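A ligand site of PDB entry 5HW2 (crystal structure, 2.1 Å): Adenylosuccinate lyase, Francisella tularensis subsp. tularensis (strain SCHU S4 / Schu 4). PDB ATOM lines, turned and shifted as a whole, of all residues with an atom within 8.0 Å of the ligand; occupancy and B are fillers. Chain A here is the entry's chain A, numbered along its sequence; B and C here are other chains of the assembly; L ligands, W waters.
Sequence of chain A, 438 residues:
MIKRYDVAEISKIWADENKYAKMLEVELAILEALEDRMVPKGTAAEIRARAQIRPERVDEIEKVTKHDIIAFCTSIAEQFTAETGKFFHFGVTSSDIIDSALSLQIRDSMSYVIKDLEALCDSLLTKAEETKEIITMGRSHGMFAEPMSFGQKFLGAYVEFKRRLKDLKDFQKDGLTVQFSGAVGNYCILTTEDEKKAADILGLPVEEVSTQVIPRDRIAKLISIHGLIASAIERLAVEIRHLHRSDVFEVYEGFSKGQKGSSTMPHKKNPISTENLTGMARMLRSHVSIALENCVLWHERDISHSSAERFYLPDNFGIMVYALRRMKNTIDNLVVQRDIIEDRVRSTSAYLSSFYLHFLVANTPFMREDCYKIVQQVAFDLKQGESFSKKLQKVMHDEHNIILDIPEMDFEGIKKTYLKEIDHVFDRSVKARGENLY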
ATOM      1  N   GLU A  27      10.461 -28.634   0.579  1.00  0.00           N
ATOM      2  CA  GLU A  27      10.022 -27.884   1.752  1.00  0.00           C
ATOM      3  C   GLU A  27       8.517 -27.965   1.932  1.00  0.00           C
ATOM      4  O   GLU A  27       8.026 -28.067   3.066  1.00  0.00           O
ATOM      5  CB  GLU A  27      10.464 -26.419   1.630  1.00  0.00           C
ATOM      6  CG  GLU A  27      11.948 -26.181   1.864  1.00  0.00           C
ATOM      7  CD  GLU A  27      12.304 -26.094   3.335  1.00  0.00           C
ATOM      8  OE1 GLU A  27      11.456 -26.447   4.186  1.00  0.00           O
ATOM      9  OE2 GLU A  27      13.431 -25.657   3.643  1.00  0.00           O
ATOM     10  N   HIS A  67      25.238 -18.856   4.569  1.00  0.00           N
ATOM     11  CA  HIS A  67      24.506 -20.111   4.663  1.00  0.00           C
ATOM     12  C   HIS A  67      23.467 -20.148   3.550  1.00  0.00           C
ATOM     13  O   HIS A  67      22.547 -19.325   3.534  1.00  0.00           O
ATOM     14  CB  HIS A  67      23.846 -20.269   6.031  1.00  0.00           C
ATOM     15  CG  HIS A  67      23.420 -21.673   6.339  1.00  0.00           C
ATOM     16  ND1 HIS A  67      22.308 -22.254   5.773  1.00  0.00           N
ATOM     17  CD2 HIS A  67      23.950 -22.597   7.174  1.00  0.00           C
ATOM     18  CE1 HIS A  67      22.177 -23.486   6.233  1.00  0.00           C
ATOM     19  NE2 HIS A  67      23.164 -23.727   7.081  1.00  0.00           N
ATOM     20  N   ASP A  68      23.611 -21.103   2.631  1.00  0.00           N
ATOM     21  CA  ASP A  68      22.780 -21.119   1.432  1.00  0.00           C
ATOM     22  C   ASP A  68      21.324 -21.416   1.772  1.00  0.00           C
ATOM     23  O   ASP A  68      20.407 -20.832   1.157  1.00  0.00           O
ATOM     24  CB  ASP A  68      23.321 -22.147   0.436  1.00  0.00           C
ATOM     25  CG  ASP A  68      23.439 -23.531   1.033  1.00  0.00           C
ATOM     26  OD1 ASP A  68      23.702 -23.639   2.244  1.00  0.00           O
ATOM     27  OD2 ASP A  68      23.266 -24.516   0.283  1.00  0.00           O
ATOM     28  N   ILE A  69      21.073 -22.299   2.730  1.00  0.00           N
ATOM     29  CA  ILE A  69      19.700 -22.709   3.023  1.00  0.00           C
ATOM     30  C   ILE A  69      18.972 -21.634   3.834  1.00  0.00           C
ATOM     31  O   ILE A  69      17.771 -21.420   3.652  1.00  0.00           O
ATOM     32  CB  ILE A  69      19.694 -24.063   3.729  1.00  0.00           C
ATOM     33  CG1 ILE A  69      20.362 -25.108   2.848  1.00  0.00           C
ATOM     34  CG2 ILE A  69      18.272 -24.502   4.047  1.00  0.00           C
ATOM     35  CD1 ILE A  69      19.796 -25.158   1.437  1.00  0.00           C
ATOM     36  N   ILE A  70      19.684 -20.956   4.733  1.00  0.00           N
ATOM     37  CA  ILE A  70      19.092 -19.822   5.433  1.00  0.00           C
ATOM     38  C   ILE A  70      18.705 -18.729   4.439  1.00  0.00           C
ATOM     39  O   ILE A  70      17.651 -18.104   4.562  1.00  0.00           O
ATOM     40  CB  ILE A  70      20.058 -19.291   6.506  1.00  0.00           C
ATOM     41  CG1 ILE A  70      20.295 -20.366   7.578  1.00  0.00           C
ATOM     42  CG2 ILE A  70      19.507 -18.020   7.150  1.00  0.00           C
ATOM     43  CD1 ILE A  70      21.278 -19.946   8.654  1.00  0.00           C
ATOM     44  N   CYS A  73      15.645 -19.993   2.617  1.00  0.00           N
ATOM     45  CA  CYS A  73      14.438 -19.910   3.425  1.00  0.00           C
ATOM     46  C   CYS A  73      13.952 -18.470   3.538  1.00  0.00           C
ATOM     47  O   CYS A  73      12.748 -18.207   3.457  1.00  0.00           O
ATOM     48  CB  CYS A  73      14.681 -20.504   4.810  1.00  0.00           C
ATOM     49  SG  CYS A  73      14.898 -22.290   4.810  1.00  0.00           S
ATOM     50  N   HIS A  89      10.107 -24.604   6.840  1.00  0.00           N
ATOM     51  CA  HIS A  89      11.407 -25.144   7.257  1.00  0.00           C
ATOM     52  C   HIS A  89      11.458 -25.291   8.775  1.00  0.00           C
ATOM     53  O   HIS A  89      12.206 -24.622   9.487  1.00  0.00           O
ATOM     54  CB  HIS A  89      12.547 -24.252   6.746  1.00  0.00           C
ATOM     55  CG  HIS A  89      13.894 -24.892   6.860  1.00  0.00           C
ATOM     56  ND1 HIS A  89      14.515 -25.518   5.802  1.00  0.00           N
ATOM     57  CD2 HIS A  89      14.747 -25.000   7.906  1.00  0.00           C
ATOM     58  CE1 HIS A  89      15.692 -25.977   6.190  1.00  0.00           C
ATOM     59  NE2 HIS A  89      15.848 -25.684   7.466  1.00  0.00           N
ATOM     60  N   PHE A  90      10.613 -26.209   9.262  1.00  0.00           N
ATOM     61  CA  PHE A  90      10.449 -26.466  10.684  1.00  0.00           C
ATOM     62  C   PHE A  90      10.661 -27.948  10.936  1.00  0.00           C
ATOM     63  O   PHE A  90      10.036 -28.792  10.285  1.00  0.00           O
ATOM     64  CB  PHE A  90       9.059 -26.029  11.159  1.00  0.00           C
ATOM     65  CG  PHE A  90       8.647 -26.618  12.467  1.00  0.00           C
ATOM     66  CD1 PHE A  90       9.095 -26.071  13.663  1.00  0.00           C
ATOM     67  CD2 PHE A  90       7.790 -27.707  12.520  1.00  0.00           C
ATOM     68  CE1 PHE A  90       8.704 -26.616  14.880  1.00  0.00           C
ATOM     69  CE2 PHE A  90       7.396 -28.246  13.728  1.00  0.00           C
ATOM     70  CZ  PHE A  90       7.857 -27.706  14.904  1.00  0.00           C
ATOM     71  N   GLY A  91      11.549 -28.267  11.884  1.00  0.00           N
ATOM     72  CA  GLY A  91      11.841 -29.632  12.248  1.00  0.00           C
ATOM     73  C   GLY A  91      12.914 -30.307  11.399  1.00  0.00           C
ATOM     74  O   GLY A  91      13.653 -31.147  11.905  1.00  0.00           O
ATOM     75  N   VAL A  92      12.995 -29.948  10.125  1.00  0.00           N
ATOM     76  CA  VAL A  92      14.003 -30.514   9.241  1.00  0.00           C
ATOM     77  C   VAL A  92      15.336 -29.815   9.469  1.00  0.00           C
ATOM     78  O   VAL A  92      15.398 -28.666   9.918  1.00  0.00           O
ATOM     79  CB  VAL A  92      13.565 -30.395   7.761  1.00  0.00           C
ATOM     80  CG1 VAL A  92      12.370 -31.282   7.484  1.00  0.00           C
ATOM     81  CG2 VAL A  92      13.262 -28.956   7.421  1.00  0.00           C
ATOM     82  N   THR A  93      16.421 -30.525   9.176  1.00  0.00           N
ATOM     83  CA  THR A  93      17.740 -29.908   9.108  1.00  0.00           C
ATOM     84  C   THR A  93      17.985 -29.441   7.668  1.00  0.00           C
ATOM     85  O   THR A  93      17.170 -29.656   6.772  1.00  0.00           O
ATOM     86  CB  THR A  93      18.821 -30.867   9.580  1.00  0.00           C
ATOM     87  OG1 THR A  93      20.054 -30.155   9.755  1.00  0.00           O
ATOM     88  CG2 THR A  93      19.039 -31.975   8.558  1.00  0.00           C
ATOM     89  N   SER A  94      19.132 -28.788   7.453  1.00  0.00           N
ATOM     90  CA  SER A  94      19.435 -28.265   6.122  1.00  0.00           C
ATOM     91  C   SER A  94      19.529 -29.386   5.100  1.00  0.00           C
ATOM     92  O   SER A  94      18.846 -29.343   4.063  1.00  0.00           O
ATOM     93  CB  SER A  94      20.732 -27.456   6.160  1.00  0.00           C
ATOM     94  OG  SER A  94      20.586 -26.309   6.985  1.00  0.00           O
ATOM     95  N   SER A  95      20.344 -30.400   5.370  1.00  0.00           N
ATOM     96  CA  SER A  95      20.556 -31.483   4.424  1.00  0.00           C
ATOM     97  C   SER A  95      19.306 -32.308   4.154  1.00  0.00           C
ATOM     98  O   SER A  95      19.287 -33.072   3.174  1.00  0.00           O
ATOM     99  CB  SER A  95      21.689 -32.391   4.895  1.00  0.00           C
ATOM    100  OG  SER A  95      22.939 -31.728   4.806  1.00  0.00           O
ATOM    101  N   ASP A  96      18.272 -32.209   4.995  1.00  0.00           N
ATOM    102  CA  ASP A  96      16.989 -32.813   4.646  1.00  0.00           C
ATOM    103  C   ASP A  96      16.463 -32.225   3.349  1.00  0.00           C
ATOM    104  O   ASP A  96      15.922 -32.955   2.503  1.00  0.00           O
ATOM    105  CB  ASP A  96      15.976 -32.608   5.771  1.00  0.00           C
ATOM    106  CG  ASP A  96      16.288 -33.446   7.001  1.00  0.00           C
ATOM    107  OD1 ASP A  96      16.878 -34.536   6.847  1.00  0.00           O
ATOM    108  OD2 ASP A  96      15.914 -33.028   8.115  1.00  0.00           O
ATOM    109  N   ILE A  97      16.611 -30.917   3.169  1.00  0.00           N
ATOM    110  CA  ILE A  97      16.161 -30.262   1.943  1.00  0.00           C
ATOM    111  C   ILE A  97      17.236 -30.309   0.852  1.00  0.00           C
ATOM    112  O   ILE A  97      16.907 -30.408  -0.333  1.00  0.00           O
ATOM    113  CB  ILE A  97      15.753 -28.811   2.252  1.00  0.00           C
ATOM    114  CG1 ILE A  97      14.863 -28.752   3.502  1.00  0.00           C
ATOM    115  CG2 ILE A  97      15.032 -28.197   1.052  1.00  0.00           C
ATOM    116  CD1 ILE A  97      13.528 -29.458   3.344  1.00  0.00           C
ATOM    117  N   ALA A 183      18.223 -33.635  12.367  1.00  0.00           N
ATOM    118  CA  ALA A 183      19.601 -33.167  12.506  1.00  0.00           C
ATOM    119  C   ALA A 183      20.609 -34.284  12.259  1.00  0.00           C
ATOM    120  O   ALA A 183      21.423 -34.208  11.333  1.00  0.00           O
ATOM    121  CB  ALA A 183      19.812 -32.549  13.889  1.00  0.00           C
ATOM    122  N   GLN A 212      23.020 -37.159   9.147  1.00  0.00           N
ATOM    123  CA  GLN A 212      22.583 -35.812   8.837  1.00  0.00           C
ATOM    124  C   GLN A 212      22.290 -35.674   7.353  1.00  0.00           C
ATOM    125  O   GLN A 212      21.348 -34.973   6.960  1.00  0.00           O
ATOM    126  CB  GLN A 212      23.636 -34.792   9.267  1.00  0.00           C
ATOM    127  CG  GLN A 212      23.338 -33.365   8.821  1.00  0.00           C
ATOM    128  CD  GLN A 212      23.686 -32.336   9.872  1.00  0.00           C
ATOM    129  OE1 GLN A 212      24.178 -31.249   9.550  1.00  0.00           O
ATOM    130  NE2 GLN A 212      23.416 -32.653  11.129  1.00  0.00           N
ATOM    131  N   ARG A 301      27.854 -36.119   9.403  1.00  0.00           N
ATOM    132  CA  ARG A 301      28.066 -35.399   8.146  1.00  0.00           C
ATOM    133  C   ARG A 301      29.336 -34.560   8.163  1.00  0.00           C
ATOM    134  O   ARG A 301      29.810 -34.142   9.215  1.00  0.00           O
ATOM    135  CB  ARG A 301      26.888 -34.468   7.814  1.00  0.00           C
ATOM    136  CG  ARG A 301      27.062 -33.049   8.318  1.00  0.00           C
ATOM    137  CD  ARG A 301      26.367 -32.057   7.412  1.00  0.00           C
ATOM    138  NE  ARG A 301      26.938 -32.066   6.076  1.00  0.00           N
ATOM    139  CZ  ARG A 301      26.339 -31.544   5.008  1.00  0.00           C
ATOM    140  NH1 ARG A 301      25.143 -30.984   5.133  1.00  0.00           N
ATOM    141  NH2 ARG A 301      26.922 -31.597   3.812  1.00  0.00           N
ATOM    142  N   PRO B 266      22.131 -18.890  16.715  1.00  0.00           N
ATOM    143  CA  PRO B 266      22.430 -18.640  15.301  1.00  0.00           C
ATOM    144  C   PRO B 266      23.923 -18.568  15.023  1.00  0.00           C
ATOM    145  O   PRO B 266      24.345 -18.723  13.874  1.00  0.00           O
ATOM    146  CB  PRO B 266      21.767 -17.285  15.052  1.00  0.00           C
ATOM    147  CG  PRO B 266      21.825 -16.605  16.369  1.00  0.00           C
ATOM    148  CD  PRO B 266      21.630 -17.689  17.397  1.00  0.00           C
ATOM    149  N   LYS B 268      27.223 -20.375  15.526  1.00  0.00           N
ATOM    150  CA  LYS B 268      27.848 -21.649  15.858  1.00  0.00           C
ATOM    151  C   LYS B 268      29.208 -21.739  15.171  1.00  0.00           C
ATOM    152  O   LYS B 268      29.406 -21.185  14.090  1.00  0.00           O
ATOM    153  CB  LYS B 268      26.971 -22.827  15.431  1.00  0.00           C
ATOM    154  N   ASN B 270      31.882 -23.935  13.217  1.00  0.00           N
ATOM    155  CA  ASN B 270      31.897 -25.087  12.327  1.00  0.00           C
ATOM    156  C   ASN B 270      33.068 -24.919  11.374  1.00  0.00           C
ATOM    157  O   ASN B 270      33.349 -23.799  10.941  1.00  0.00           O
ATOM    158  CB  ASN B 270      30.586 -25.213  11.527  1.00  0.00           C
ATOM    159  CG  ASN B 270      29.424 -25.688  12.384  1.00  0.00           C
ATOM    160  OD1 ASN B 270      29.568 -26.600  13.196  1.00  0.00           O
ATOM    161  ND2 ASN B 270      28.270 -25.069  12.189  1.00  0.00           N
ATOM    162  N   SER C 140      27.887 -33.258  13.564  1.00  0.00           N
ATOM    163  CA  SER C 140      27.918 -32.749  12.202  1.00  0.00           C
ATOM    164  C   SER C 140      29.075 -31.765  12.089  1.00  0.00           C
ATOM    165  O   SER C 140      29.237 -30.898  12.957  1.00  0.00           O
ATOM    166  CB  SER C 140      26.599 -32.064  11.838  1.00  0.00           C
ATOM    167  OG  SER C 140      26.369 -30.927  12.652  1.00  0.00           O
ATOM    168  N   HIS C 141      29.880 -31.925  11.030  1.00  0.00           N
ATOM    169  CA  HIS C 141      31.110 -31.147  10.856  1.00  0.00           C
ATOM    170  C   HIS C 141      32.083 -31.357  12.006  1.00  0.00           C
ATOM    171  O   HIS C 141      32.902 -30.486  12.313  1.00  0.00           O
ATOM    172  CB  HIS C 141      30.811 -29.655  10.678  1.00  0.00           C
ATOM    173  CG  HIS C 141      29.715 -29.374   9.698  1.00  0.00           C
ATOM    174  ND1 HIS C 141      29.922 -29.312   8.340  1.00  0.00           N
ATOM    175  CD2 HIS C 141      28.398 -29.121   9.882  1.00  0.00           C
ATOM    176  CE1 HIS C 141      28.781 -29.043   7.732  1.00  0.00           C
ATOM    177  NE2 HIS C 141      27.840 -28.920   8.650  1.00  0.00           N
ATOM    178  N   SER C 354      17.426 -25.649  20.786  1.00  0.00           N
ATOM    179  CA  SER C 354      16.631 -25.946  19.594  1.00  0.00           C
ATOM    180  C   SER C 354      15.403 -26.793  19.944  1.00  0.00           C
ATOM    181  O   SER C 354      14.373 -26.682  19.266  1.00  0.00           O
ATOM    182  CB  SER C 354      17.490 -26.665  18.554  1.00  0.00           C
ATOM    183  OG  SER C 354      16.740 -26.955  17.385  1.00  0.00           O
ATOM    184  N   LEU C 357      12.873 -24.483  21.635  1.00  0.00           N
ATOM    185  CA  LEU C 357      12.421 -23.501  20.659  1.00  0.00           C
ATOM    186  C   LEU C 357      11.268 -24.058  19.820  1.00  0.00           C
ATOM    187  O   LEU C 357      10.195 -23.449  19.735  1.00  0.00           O
ATOM    188  CB  LEU C 357      13.586 -23.087  19.754  1.00  0.00           C
ATOM    189  CG  LEU C 357      13.330 -22.622  18.361  1.00  0.00           C
ATOM    190  CD1 LEU C 357      12.667 -21.317  18.350  1.00  0.00           C
ATOM    191  CD2 LEU C 357      14.608 -22.561  17.561  1.00  0.00           C
ATOM    192  N   HIS C 358      11.480 -25.215  19.194  1.00  0.00           N
ATOM    193  CA  HIS C 358      10.419 -25.844  18.413  1.00  0.00           C
ATOM    194  C   HIS C 358       9.245 -26.258  19.273  1.00  0.00           C
ATOM    195  O   HIS C 358       8.139 -26.444  18.752  1.00  0.00           O
ATOM    196  CB  HIS C 358      10.971 -27.050  17.650  1.00  0.00           C
ATOM    197  CG  HIS C 358      12.053 -26.706  16.661  1.00  0.00           C
ATOM    198  ND1 HIS C 358      13.327 -26.335  17.047  1.00  0.00           N
ATOM    199  CD2 HIS C 358      12.048 -26.662  15.308  1.00  0.00           C
ATOM    200  CE1 HIS C 358      14.058 -26.095  15.979  1.00  0.00           C
ATOM    201  NE2 HIS C 358      13.301 -26.287  14.906  1.00  0.00           N
HETATM  202  O1  LIG L   1      17.898 -24.865  11.087  1.00  0.00           O
HETATM  203  C1  LIG L   1      18.317 -25.536  10.113  1.00  0.00           C
HETATM  204  O2  LIG L   1      17.575 -26.281   9.440  1.00  0.00           O
HETATM  205  C2  LIG L   1      19.744 -25.451   9.757  1.00  0.00           C
HETATM  206  C3  LIG L   1      20.674 -25.442  10.711  1.00  0.00           C
HETATM  207  C4  LIG L   1      22.089 -25.352  10.327  1.00  0.00           C
HETATM  208  O3  LIG L   1      22.476 -24.402   9.624  1.00  0.00           O
HETATM  209  O4  LIG L   1      22.869 -26.236  10.745  1.00  0.00           O
HETATM  210  O   HOH W   1      24.425 -28.993  12.038  1.00  0.00           O
HETATM  211  O   HOH W   2      25.220 -26.701  11.845  1.00  0.00           O
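Water W2 lies within hydrogen-bond range of O4 of the ligand (2.6 Å) and ND2 of Asn 270 of chain B (3.5 Å).
Water W1 lies within hydrogen-bond range of OG of Ser 140 of chain C (2.8 Å), OE1 of Gln 212 (3.4 Å) and O4 of the ligand (3.4 Å).
An oxygen (O2) of the ligand sits close to the backbone carbonyl oxygen of Val 92 (3.3 Å).
Residues that only touch the ligand: Thr 93 and Ser 94.
A ring nitrogen (ND1) of His 89 lies within hydrogen-bond range of the side-chain sulfur (SG) of Cys 73, at 3.4 Å.
OE2 of Glu 27 is in hydrogen-bond range of ND1 of His 89, at 2.4 Å.
The backbone NH (N) of Ile 70 is in hydrogen-bond range of a ring nitrogen (ND1) of His 67, 3.1 Å away.
ND1 of His 67 sits at hydrogen-bond distance from N of Ile 69 (3.3 Å).
The backbone NH (N) of Thr 93 sits at hydrogen-bond distance from the side-chain carboxylate (OD2) of Asp 96 (2.8 Å).
A ring nitrogen (NE2) of His 89 lies within hydrogen-bond range of an oxygen (O2) of the ligand (2.7 Å).
A ring nitrogen (NE2) of His 67 sits at hydrogen-bond distance from an oxygen (O3) of the ligand (2.7 Å).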
